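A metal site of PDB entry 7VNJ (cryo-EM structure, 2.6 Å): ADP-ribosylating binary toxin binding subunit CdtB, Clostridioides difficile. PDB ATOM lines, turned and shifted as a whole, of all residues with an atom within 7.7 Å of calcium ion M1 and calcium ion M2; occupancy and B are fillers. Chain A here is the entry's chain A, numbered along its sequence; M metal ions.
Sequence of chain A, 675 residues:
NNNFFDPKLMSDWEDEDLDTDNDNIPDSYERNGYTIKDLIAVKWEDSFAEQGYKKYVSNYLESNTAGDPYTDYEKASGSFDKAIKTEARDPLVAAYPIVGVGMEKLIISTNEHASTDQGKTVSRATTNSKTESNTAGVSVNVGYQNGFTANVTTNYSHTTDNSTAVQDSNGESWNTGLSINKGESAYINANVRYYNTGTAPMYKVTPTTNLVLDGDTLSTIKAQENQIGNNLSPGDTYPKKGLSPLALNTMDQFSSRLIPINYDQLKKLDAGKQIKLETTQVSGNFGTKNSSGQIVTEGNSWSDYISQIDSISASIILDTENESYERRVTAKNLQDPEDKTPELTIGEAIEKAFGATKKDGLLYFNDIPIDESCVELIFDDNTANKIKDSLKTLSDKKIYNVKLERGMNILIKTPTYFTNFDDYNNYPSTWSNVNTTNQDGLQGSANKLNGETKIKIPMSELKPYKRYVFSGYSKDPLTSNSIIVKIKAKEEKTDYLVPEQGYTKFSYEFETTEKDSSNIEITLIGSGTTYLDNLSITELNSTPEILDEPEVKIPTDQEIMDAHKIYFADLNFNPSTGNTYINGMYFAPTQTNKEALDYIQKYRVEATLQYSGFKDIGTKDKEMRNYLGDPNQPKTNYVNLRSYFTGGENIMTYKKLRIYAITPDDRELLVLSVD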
ATOM      1  N   LEU A  18      18.028 -24.282 -17.285  1.00  0.00           N
ATOM      2  CA  LEU A  18      18.110 -25.013 -18.538  1.00  0.00           C
ATOM      3  C   LEU A  18      18.870 -24.175 -19.564  1.00  0.00           C
ATOM      4  O   LEU A  18      18.517 -23.022 -19.811  1.00  0.00           O
ATOM      5  CB  LEU A  18      16.716 -25.351 -19.062  1.00  0.00           C
ATOM      6  CG  LEU A  18      16.636 -26.197 -20.336  1.00  0.00           C
ATOM      7  CD1 LEU A  18      17.287 -27.543 -20.110  1.00  0.00           C
ATOM      8  CD2 LEU A  18      15.197 -26.350 -20.767  1.00  0.00           C
ATOM      9  N   ASP A  19      19.897 -24.773 -20.158  1.00  0.00           N
ATOM     10  CA  ASP A  19      20.779 -24.089 -21.110  1.00  0.00           C
ATOM     11  C   ASP A  19      20.863 -24.956 -22.363  1.00  0.00           C
ATOM     12  O   ASP A  19      21.731 -25.832 -22.466  1.00  0.00           O
ATOM     13  CB  ASP A  19      22.146 -23.842 -20.500  1.00  0.00           C
ATOM     14  CG  ASP A  19      22.938 -22.789 -21.241  1.00  0.00           C
ATOM     15  OD1 ASP A  19      22.432 -22.266 -22.252  1.00  0.00           O
ATOM     16  OD2 ASP A  19      24.073 -22.486 -20.816  1.00  0.00           O
ATOM     17  N   THR A  20      19.960 -24.730 -23.314  1.00  0.00           N
ATOM     18  CA  THR A  20      19.882 -25.581 -24.490  1.00  0.00           C
ATOM     19  C   THR A  20      21.103 -25.420 -25.388  1.00  0.00           C
ATOM     20  O   THR A  20      21.657 -26.413 -25.876  1.00  0.00           O
ATOM     21  CB  THR A  20      18.599 -25.292 -25.271  1.00  0.00           C
ATOM     22  OG1 THR A  20      17.483 -25.305 -24.363  1.00  0.00           O
ATOM     23  CG2 THR A  20      18.381 -26.335 -26.336  1.00  0.00           C
ATOM     24  N   ASP A  21      21.533 -24.183 -25.620  1.00  0.00           N
ATOM     25  CA  ASP A  21      22.657 -23.928 -26.515  1.00  0.00           C
ATOM     26  C   ASP A  21      24.002 -23.955 -25.818  1.00  0.00           C
ATOM     27  O   ASP A  21      25.034 -23.854 -26.495  1.00  0.00           O
ATOM     28  CB  ASP A  21      22.474 -22.577 -27.228  1.00  0.00           C
ATOM     29  CG  ASP A  21      22.213 -21.447 -26.267  1.00  0.00           C
ATOM     30  OD1 ASP A  21      22.236 -21.674 -25.045  1.00  0.00           O
ATOM     31  OD2 ASP A  21      21.993 -20.316 -26.734  1.00  0.00           O
ATOM     32  N   ASN A  22      24.018 -24.079 -24.492  1.00  0.00           N
ATOM     33  CA  ASN A  22      25.257 -24.214 -23.710  1.00  0.00           C
ATOM     34  C   ASN A  22      26.151 -22.980 -23.849  1.00  0.00           C
ATOM     35  O   ASN A  22      27.359 -23.089 -24.054  1.00  0.00           O
ATOM     36  CB  ASN A  22      26.014 -25.481 -24.099  1.00  0.00           C
ATOM     37  CG  ASN A  22      25.301 -26.741 -23.646  1.00  0.00           C
ATOM     38  OD1 ASN A  22      25.108 -26.967 -22.457  1.00  0.00           O
ATOM     39  ND2 ASN A  22      24.915 -27.580 -24.607  1.00  0.00           N
ATOM     40  N   ASP A  23      25.546 -21.803 -23.721  1.00  0.00           N
ATOM     41  CA  ASP A  23      26.301 -20.553 -23.759  1.00  0.00           C
ATOM     42  C   ASP A  23      26.360 -19.882 -22.392  1.00  0.00           C
ATOM     43  O   ASP A  23      26.581 -18.663 -22.315  1.00  0.00           O
ATOM     44  CB  ASP A  23      25.702 -19.607 -24.793  1.00  0.00           C
ATOM     45  CG  ASP A  23      24.258 -19.239 -24.512  1.00  0.00           C
ATOM     46  OD1 ASP A  23      23.678 -19.771 -23.549  1.00  0.00           O
ATOM     47  OD2 ASP A  23      23.700 -18.421 -25.272  1.00  0.00           O
ATOM     48  N   ASN A  24      26.137 -20.640 -21.315  1.00  0.00           N
ATOM     49  CA  ASN A  24      26.223 -20.180 -19.928  1.00  0.00           C
ATOM     50  C   ASN A  24      25.102 -19.225 -19.533  1.00  0.00           C
ATOM     51  O   ASN A  24      25.200 -18.591 -18.481  1.00  0.00           O
ATOM     52  CB  ASN A  24      27.571 -19.536 -19.607  1.00  0.00           C
ATOM     53  CG  ASN A  24      28.706 -20.528 -19.603  1.00  0.00           C
ATOM     54  OD1 ASN A  24      28.510 -21.717 -19.365  1.00  0.00           O
ATOM     55  ND2 ASN A  24      29.911 -20.046 -19.881  1.00  0.00           N
ATOM     56  N   ILE A  25      24.060 -19.094 -20.344  1.00  0.00           N
ATOM     57  CA  ILE A  25      22.911 -18.258 -20.029  1.00  0.00           C
ATOM     58  C   ILE A  25      21.666 -19.127 -20.100  1.00  0.00           C
ATOM     59  O   ILE A  25      21.434 -19.773 -21.126  1.00  0.00           O
ATOM     60  CB  ILE A  25      22.773 -17.053 -20.976  1.00  0.00           C
ATOM     61  CG1 ILE A  25      24.123 -16.359 -21.163  1.00  0.00           C
ATOM     62  CG2 ILE A  25      21.758 -16.065 -20.434  1.00  0.00           C
ATOM     63  CD1 ILE A  25      24.138 -15.366 -22.289  1.00  0.00           C
ATOM     64  N   PRO A  26      20.852 -19.193 -19.045  1.00  0.00           N
ATOM     65  CA  PRO A  26      19.664 -20.047 -19.091  1.00  0.00           C
ATOM     66  C   PRO A  26      18.659 -19.570 -20.128  1.00  0.00           C
ATOM     67  O   PRO A  26      18.644 -18.405 -20.524  1.00  0.00           O
ATOM     68  CB  PRO A  26      19.096 -19.925 -17.670  1.00  0.00           C
ATOM     69  CG  PRO A  26      20.240 -19.488 -16.829  1.00  0.00           C
ATOM     70  CD  PRO A  26      21.076 -18.617 -17.712  1.00  0.00           C
ATOM     71  N   ASP A  27      17.827 -20.513 -20.583  1.00  0.00           N
ATOM     72  CA  ASP A  27      16.872 -20.212 -21.644  1.00  0.00           C
ATOM     73  C   ASP A  27      15.883 -19.130 -21.236  1.00  0.00           C
ATOM     74  O   ASP A  27      15.596 -18.209 -22.004  1.00  0.00           O
ATOM     75  CB  ASP A  27      16.121 -21.484 -22.041  1.00  0.00           C
ATOM     76  CG  ASP A  27      17.025 -22.510 -22.698  1.00  0.00           C
ATOM     77  OD1 ASP A  27      18.222 -22.208 -22.892  1.00  0.00           O
ATOM     78  OD2 ASP A  27      16.540 -23.611 -23.017  1.00  0.00           O
ATOM     79  N   SER A  28      15.347 -19.217 -20.016  1.00  0.00           N
ATOM     80  CA  SER A  28      14.381 -18.235 -19.565  1.00  0.00           C
ATOM     81  C   SER A  28      15.026 -16.859 -19.426  1.00  0.00           C
ATOM     82  O   SER A  28      14.377 -15.832 -19.690  1.00  0.00           O
ATOM     83  CB  SER A  28      13.753 -18.663 -18.244  1.00  0.00           C
ATOM     84  OG  SER A  28      14.752 -18.906 -17.267  1.00  0.00           O
ATOM     85  N   TYR A  29      16.289 -16.815 -19.006  1.00  0.00           N
ATOM     86  CA  TYR A  29      16.995 -15.544 -18.918  1.00  0.00           C
ATOM     87  C   TYR A  29      17.120 -14.897 -20.295  1.00  0.00           C
ATOM     88  O   TYR A  29      16.907 -13.686 -20.439  1.00  0.00           O
ATOM     89  CB  TYR A  29      18.380 -15.742 -18.298  1.00  0.00           C
ATOM     90  CG  TYR A  29      18.393 -16.028 -16.813  1.00  0.00           C
ATOM     91  CD1 TYR A  29      17.279 -16.559 -16.168  1.00  0.00           C
ATOM     92  CD2 TYR A  29      19.524 -15.783 -16.060  1.00  0.00           C
ATOM     93  CE1 TYR A  29      17.298 -16.829 -14.822  1.00  0.00           C
ATOM     94  CE2 TYR A  29      19.552 -16.045 -14.706  1.00  0.00           C
ATOM     95  CZ  TYR A  29      18.441 -16.570 -14.093  1.00  0.00           C
ATOM     96  OH  TYR A  29      18.464 -16.827 -12.750  1.00  0.00           O
ATOM     97  N   GLU A  30      17.474 -15.688 -21.308  1.00  0.00           N
ATOM     98  CA  GLU A  30      17.572 -15.148 -22.657  1.00  0.00           C
ATOM     99  C   GLU A  30      16.217 -14.692 -23.182  1.00  0.00           C
ATOM    100  O   GLU A  30      16.115 -13.668 -23.862  1.00  0.00           O
ATOM    101  CB  GLU A  30      18.177 -16.195 -23.600  1.00  0.00           C
ATOM    102  CG  GLU A  30      19.562 -16.651 -23.223  1.00  0.00           C
ATOM    103  CD  GLU A  30      20.336 -17.222 -24.403  1.00  0.00           C
ATOM    104  OE1 GLU A  30      20.566 -16.476 -25.371  1.00  0.00           O
ATOM    105  OE2 GLU A  30      20.689 -18.410 -24.351  1.00  0.00           O
ATOM    106  N   TYR A  34      18.153 -10.226 -19.161  1.00  0.00           N
ATOM    107  CA  TYR A  34      19.209 -10.511 -18.204  1.00  0.00           C
ATOM    108  C   TYR A  34      20.278  -9.445 -18.299  1.00  0.00           C
ATOM    109  O   TYR A  34      20.307  -8.639 -19.235  1.00  0.00           O
ATOM    110  CB  TYR A  34      19.816 -11.894 -18.433  1.00  0.00           C
ATOM    111  CG  TYR A  34      20.500 -12.049 -19.776  1.00  0.00           C
ATOM    112  CD1 TYR A  34      19.775 -12.345 -20.916  1.00  0.00           C
ATOM    113  CD2 TYR A  34      21.866 -11.884 -19.900  1.00  0.00           C
ATOM    114  CE1 TYR A  34      20.388 -12.480 -22.134  1.00  0.00           C
ATOM    115  CE2 TYR A  34      22.501 -12.017 -21.118  1.00  0.00           C
ATOM    116  CZ  TYR A  34      21.755 -12.316 -22.233  1.00  0.00           C
ATOM    117  OH  TYR A  34      22.368 -12.451 -23.451  1.00  0.00           O
ATOM    118  N   SER A  58      18.351 -12.436 -26.154  1.00  0.00           N
ATOM    119  CA  SER A  58      19.084 -13.136 -27.201  1.00  0.00           C
ATOM    120  C   SER A  58      18.368 -14.438 -27.536  1.00  0.00           C
ATOM    121  O   SER A  58      17.321 -14.769 -26.982  1.00  0.00           O
ATOM    122  CB  SER A  58      20.533 -13.385 -26.777  1.00  0.00           C
ATOM    123  OG  SER A  58      20.605 -14.236 -25.653  1.00  0.00           O
ATOM    124  N   ASN A  59      18.949 -15.184 -28.473  1.00  0.00           N
ATOM    125  CA  ASN A  59      18.379 -16.433 -28.954  1.00  0.00           C
ATOM    126  C   ASN A  59      18.807 -17.572 -28.050  1.00  0.00           C
ATOM    127  O   ASN A  59      19.996 -17.872 -27.934  1.00  0.00           O
ATOM    128  CB  ASN A  59      18.830 -16.675 -30.400  1.00  0.00           C
ATOM    129  CG  ASN A  59      18.063 -17.795 -31.071  1.00  0.00           C
ATOM    130  OD1 ASN A  59      17.382 -18.577 -30.423  1.00  0.00           O
ATOM    131  ND2 ASN A  59      18.170 -17.857 -32.389  1.00  0.00           N
ATOM    132  N   TYR A  60      17.842 -18.225 -27.410  1.00  0.00           N
ATOM    133  CA  TYR A  60      18.149 -19.296 -26.479  1.00  0.00           C
ATOM    134  C   TYR A  60      18.466 -20.619 -27.170  1.00  0.00           C
ATOM    135  O   TYR A  60      18.941 -21.539 -26.508  1.00  0.00           O
ATOM    136  CB  TYR A  60      17.004 -19.491 -25.487  1.00  0.00           C
ATOM    137  CG  TYR A  60      15.783 -20.201 -26.031  1.00  0.00           C
ATOM    138  CD1 TYR A  60      14.819 -19.502 -26.750  1.00  0.00           C
ATOM    139  CD2 TYR A  60      15.582 -21.551 -25.810  1.00  0.00           C
ATOM    140  CE1 TYR A  60      13.706 -20.143 -27.239  1.00  0.00           C
ATOM    141  CE2 TYR A  60      14.470 -22.200 -26.304  1.00  0.00           C
ATOM    142  CZ  TYR A  60      13.536 -21.492 -27.014  1.00  0.00           C
ATOM    143  OH  TYR A  60      12.423 -22.133 -27.504  1.00  0.00           O
ATOM    144  N   LEU A  61      18.222 -20.717 -28.471  1.00  0.00           N
ATOM    145  CA  LEU A  61      18.585 -21.901 -29.249  1.00  0.00           C
ATOM    146  C   LEU A  61      19.849 -21.705 -30.056  1.00  0.00           C
ATOM    147  O   LEU A  61      20.264 -22.628 -30.763  1.00  0.00           O
ATOM    148  CB  LEU A  61      17.432 -22.291 -30.182  1.00  0.00           C
ATOM    149  CG  LEU A  61      16.235 -22.970 -29.547  1.00  0.00           C
ATOM    150  CD1 LEU A  61      15.213 -23.342 -30.604  1.00  0.00           C
ATOM    151  CD2 LEU A  61      16.665 -24.205 -28.783  1.00  0.00           C
ATOM    152  N   GLU A  62      20.483 -20.542 -29.965  1.00  0.00           N
ATOM    153  CA  GLU A  62      21.663 -20.232 -30.763  1.00  0.00           C
ATOM    154  C   GLU A  62      22.752 -19.674 -29.857  1.00  0.00           C
ATOM    155  O   GLU A  62      22.497 -18.761 -29.064  1.00  0.00           O
ATOM    156  CB  GLU A  62      21.318 -19.223 -31.861  1.00  0.00           C
ATOM    157  CG  GLU A  62      22.475 -18.885 -32.780  1.00  0.00           C
ATOM    158  CD  GLU A  62      22.857 -20.043 -33.671  1.00  0.00           C
ATOM    159  OE1 GLU A  62      21.954 -20.735 -34.184  1.00  0.00           O
ATOM    160  OE2 GLU A  62      24.078 -20.258 -33.866  1.00  0.00           O
ATOM    161  N   SER A  63      23.962 -20.221 -29.981  1.00  0.00           N
ATOM    162  CA  SER A  63      25.068 -19.770 -29.150  1.00  0.00           C
ATOM    163  C   SER A  63      25.602 -18.417 -29.591  1.00  0.00           C
ATOM    164  O   SER A  63      26.123 -17.663 -28.773  1.00  0.00           O
ATOM    165  CB  SER A  63      26.180 -20.812 -29.162  1.00  0.00           C
ATOM    166  OG  SER A  63      27.202 -20.468 -28.245  1.00  0.00           O
ATOM    167  N   ASN A  64      25.491 -18.103 -30.883  1.00  0.00           N
ATOM    168  CA  ASN A  64      25.950 -16.834 -31.434  1.00  0.00           C
ATOM    169  C   ASN A  64      24.753 -16.202 -32.143  1.00  0.00           C
ATOM    170  O   ASN A  64      24.509 -16.456 -33.319  1.00  0.00           O
ATOM    171  CB  ASN A  64      27.119 -17.042 -32.388  1.00  0.00           C
ATOM    172  CG  ASN A  64      28.312 -17.684 -31.724  1.00  0.00           C
ATOM    173  OD1 ASN A  64      28.235 -18.815 -31.255  1.00  0.00           O
ATOM    174  ND2 ASN A  64      29.435 -16.978 -31.705  1.00  0.00           N
ATOM    175  N   THR A  65      24.018 -15.363 -31.407  1.00  0.00           N
ATOM    176  CA  THR A  65      22.788 -14.795 -31.956  1.00  0.00           C
ATOM    177  C   THR A  65      23.067 -13.923 -33.180  1.00  0.00           C
ATOM    178  O   THR A  65      22.350 -14.006 -34.185  1.00  0.00           O
ATOM    179  CB  THR A  65      22.073 -13.972 -30.881  1.00  0.00           C
ATOM    180  OG1 THR A  65      21.873 -14.783 -29.721  1.00  0.00           O
ATOM    181  CG2 THR A  65      20.726 -13.500 -31.393  1.00  0.00           C
ATOM    182  N   THR A  71      30.406 -15.473 -28.730  1.00  0.00           N
ATOM    183  CA  THR A  71      29.161 -16.012 -28.218  1.00  0.00           C
ATOM    184  C   THR A  71      28.371 -14.941 -27.479  1.00  0.00           C
ATOM    185  O   THR A  71      28.859 -13.832 -27.216  1.00  0.00           O
ATOM    186  CB  THR A  71      29.423 -17.204 -27.301  1.00  0.00           C
ATOM    187  OG1 THR A  71      29.875 -16.738 -26.027  1.00  0.00           O
ATOM    188  CG2 THR A  71      30.484 -18.104 -27.896  1.00  0.00           C
ATOM    189  N   ASP A  72      27.125 -15.281 -27.131  1.00  0.00           N
ATOM    190  CA  ASP A  72      26.264 -14.335 -26.422  1.00  0.00           C
ATOM    191  C   ASP A  72      26.859 -13.953 -25.074  1.00  0.00           C
ATOM    192  O   ASP A  72      26.867 -12.765 -24.708  1.00  0.00           O
ATOM    193  CB  ASP A  72      24.879 -14.924 -26.245  1.00  0.00           C
ATOM    194  CG  ASP A  72      24.147 -15.097 -27.558  1.00  0.00           C
ATOM    195  OD1 ASP A  72      24.618 -14.567 -28.575  1.00  0.00           O
ATOM    196  OD2 ASP A  72      23.102 -15.776 -27.572  1.00  0.00           O
ATOM    197  N   TYR A  73      27.353 -14.930 -24.322  1.00  0.00           N
ATOM    198  CA  TYR A  73      27.931 -14.630 -23.015  1.00  0.00           C
ATOM    199  C   TYR A  73      29.184 -13.778 -23.150  1.00  0.00           C
ATOM    200  O   TYR A  73      29.379 -12.833 -22.376  1.00  0.00           O
ATOM    201  CB  TYR A  73      28.249 -15.923 -22.265  1.00  0.00           C
ATOM    202  CG  TYR A  73      29.006 -15.675 -20.985  1.00  0.00           C
ATOM    203  CD1 TYR A  73      28.353 -15.220 -19.846  1.00  0.00           C
ATOM    204  CD2 TYR A  73      30.382 -15.869 -20.916  1.00  0.00           C
ATOM    205  CE1 TYR A  73      29.046 -14.984 -18.681  1.00  0.00           C
ATOM    206  CE2 TYR A  73      31.079 -15.621 -19.754  1.00  0.00           C
ATOM    207  CZ  TYR A  73      30.401 -15.188 -18.641  1.00  0.00           C
ATOM    208  OH  TYR A  73      31.085 -14.952 -17.479  1.00  0.00           O
ATOM    209  N   PRO A  91      23.935  -8.901 -27.598  1.00  0.00           N
ATOM    210  CA  PRO A  91      23.943 -10.009 -28.573  1.00  0.00           C
ATOM    211  C   PRO A  91      23.305  -9.686 -29.912  1.00  0.00           C
ATOM    212  O   PRO A  91      23.561 -10.409 -30.874  1.00  0.00           O
ATOM    213  CB  PRO A  91      23.169 -11.114 -27.840  1.00  0.00           C
ATOM    214  CG  PRO A  91      23.395 -10.818 -26.400  1.00  0.00           C
ATOM    215  CD  PRO A  91      23.401  -9.327 -26.290  1.00  0.00           C
HETATM  216 CA    CA M   1      21.299 -20.444 -23.329  1.00  0.00          CA
HETATM  217 CA    CA M   2      22.111 -17.880 -26.904  1.00  0.00          CA
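Within 4 Å of calcium ion M2: Asp 21, Asp 23, Glu 30, Asn 59, Glu 62 and Asp 72.
The backbone NH (N) of Asn 59 lies within hydrogen-bond range of the side-chain hydroxyl (OG1) of Thr 65 (3.2 Å). N of Leu 61 is in hydrogen-bond range of OD1 of Asn 59 (3.0 Å). The side-chain carboxylate (OD1) of Asp 19 sits close to the backbone NH (N) of Asn 22, 3.3 Å away. The side-chain carboxylate (OD2) of Asp 19 sits at hydrogen-bond distance from the backbone NH (N) of Asn 24, 2.8 Å away. The backbone NH (N) of Asp 72 is in hydrogen-bond range of the backbone carbonyl oxygen (O) of Ser 63 (3.1 Å). The side-chain hydroxyl (OG1) of Thr 65 lies within hydrogen-bond range of the side-chain carboxylate (OD1) of Asp 72, at 3.0 Å. The side-chain carboxylate of Asp 27 sits at hydrogen-bond distance from the backbone NH of Thr 20. N of Asp 27 lies within hydrogen-bond range of O of Leu 18.
Asp 27 touches calcium ion M1. Six residues have an atom within 4 Å of calcium ion M1: Asp 19, Asp 21, Asp 23, Ile 25, Asp 27 and Glu 30. The nearest printed residue that does not touch calcium ion M1 is Tyr 60 (4.1 Å).
Calcium ion M2 is bound by the side-chain carboxylate (OD2) of Asp 23 (2.3 Å), the backbone carbonyl oxygen (O) of Asn 59 (2.4 Å), the backbone carbonyl oxygen (O) of Glu 62 (2.4 Å), the side-chain carboxylate (OD2) of Asp 72 (2.4 Å), the side-chain carboxylate (OD2) of Asp 21 (2.4 Å) and the side-chain carboxylate (OE1) of Glu 30 (2.6 Å). Calcium ion M2 has six donor atoms within binding distance. Slightly farther from calcium ion M2 lies the side-chain carboxylate (OE2) of Glu 30 (3.0 Å).
Calcium ion M1 is bound by the backbone carbonyl oxygen of Ile 25 (2.3 Å), the side-chain carboxylate of Asp 21 (2.3 Å), the side-chain carboxylate of Glu 30 (2.4 Å), the side-chain carboxylate of Asp 19 (2.4 Å) and the side-chain carboxylate of Asp 23 (2.5 Å).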
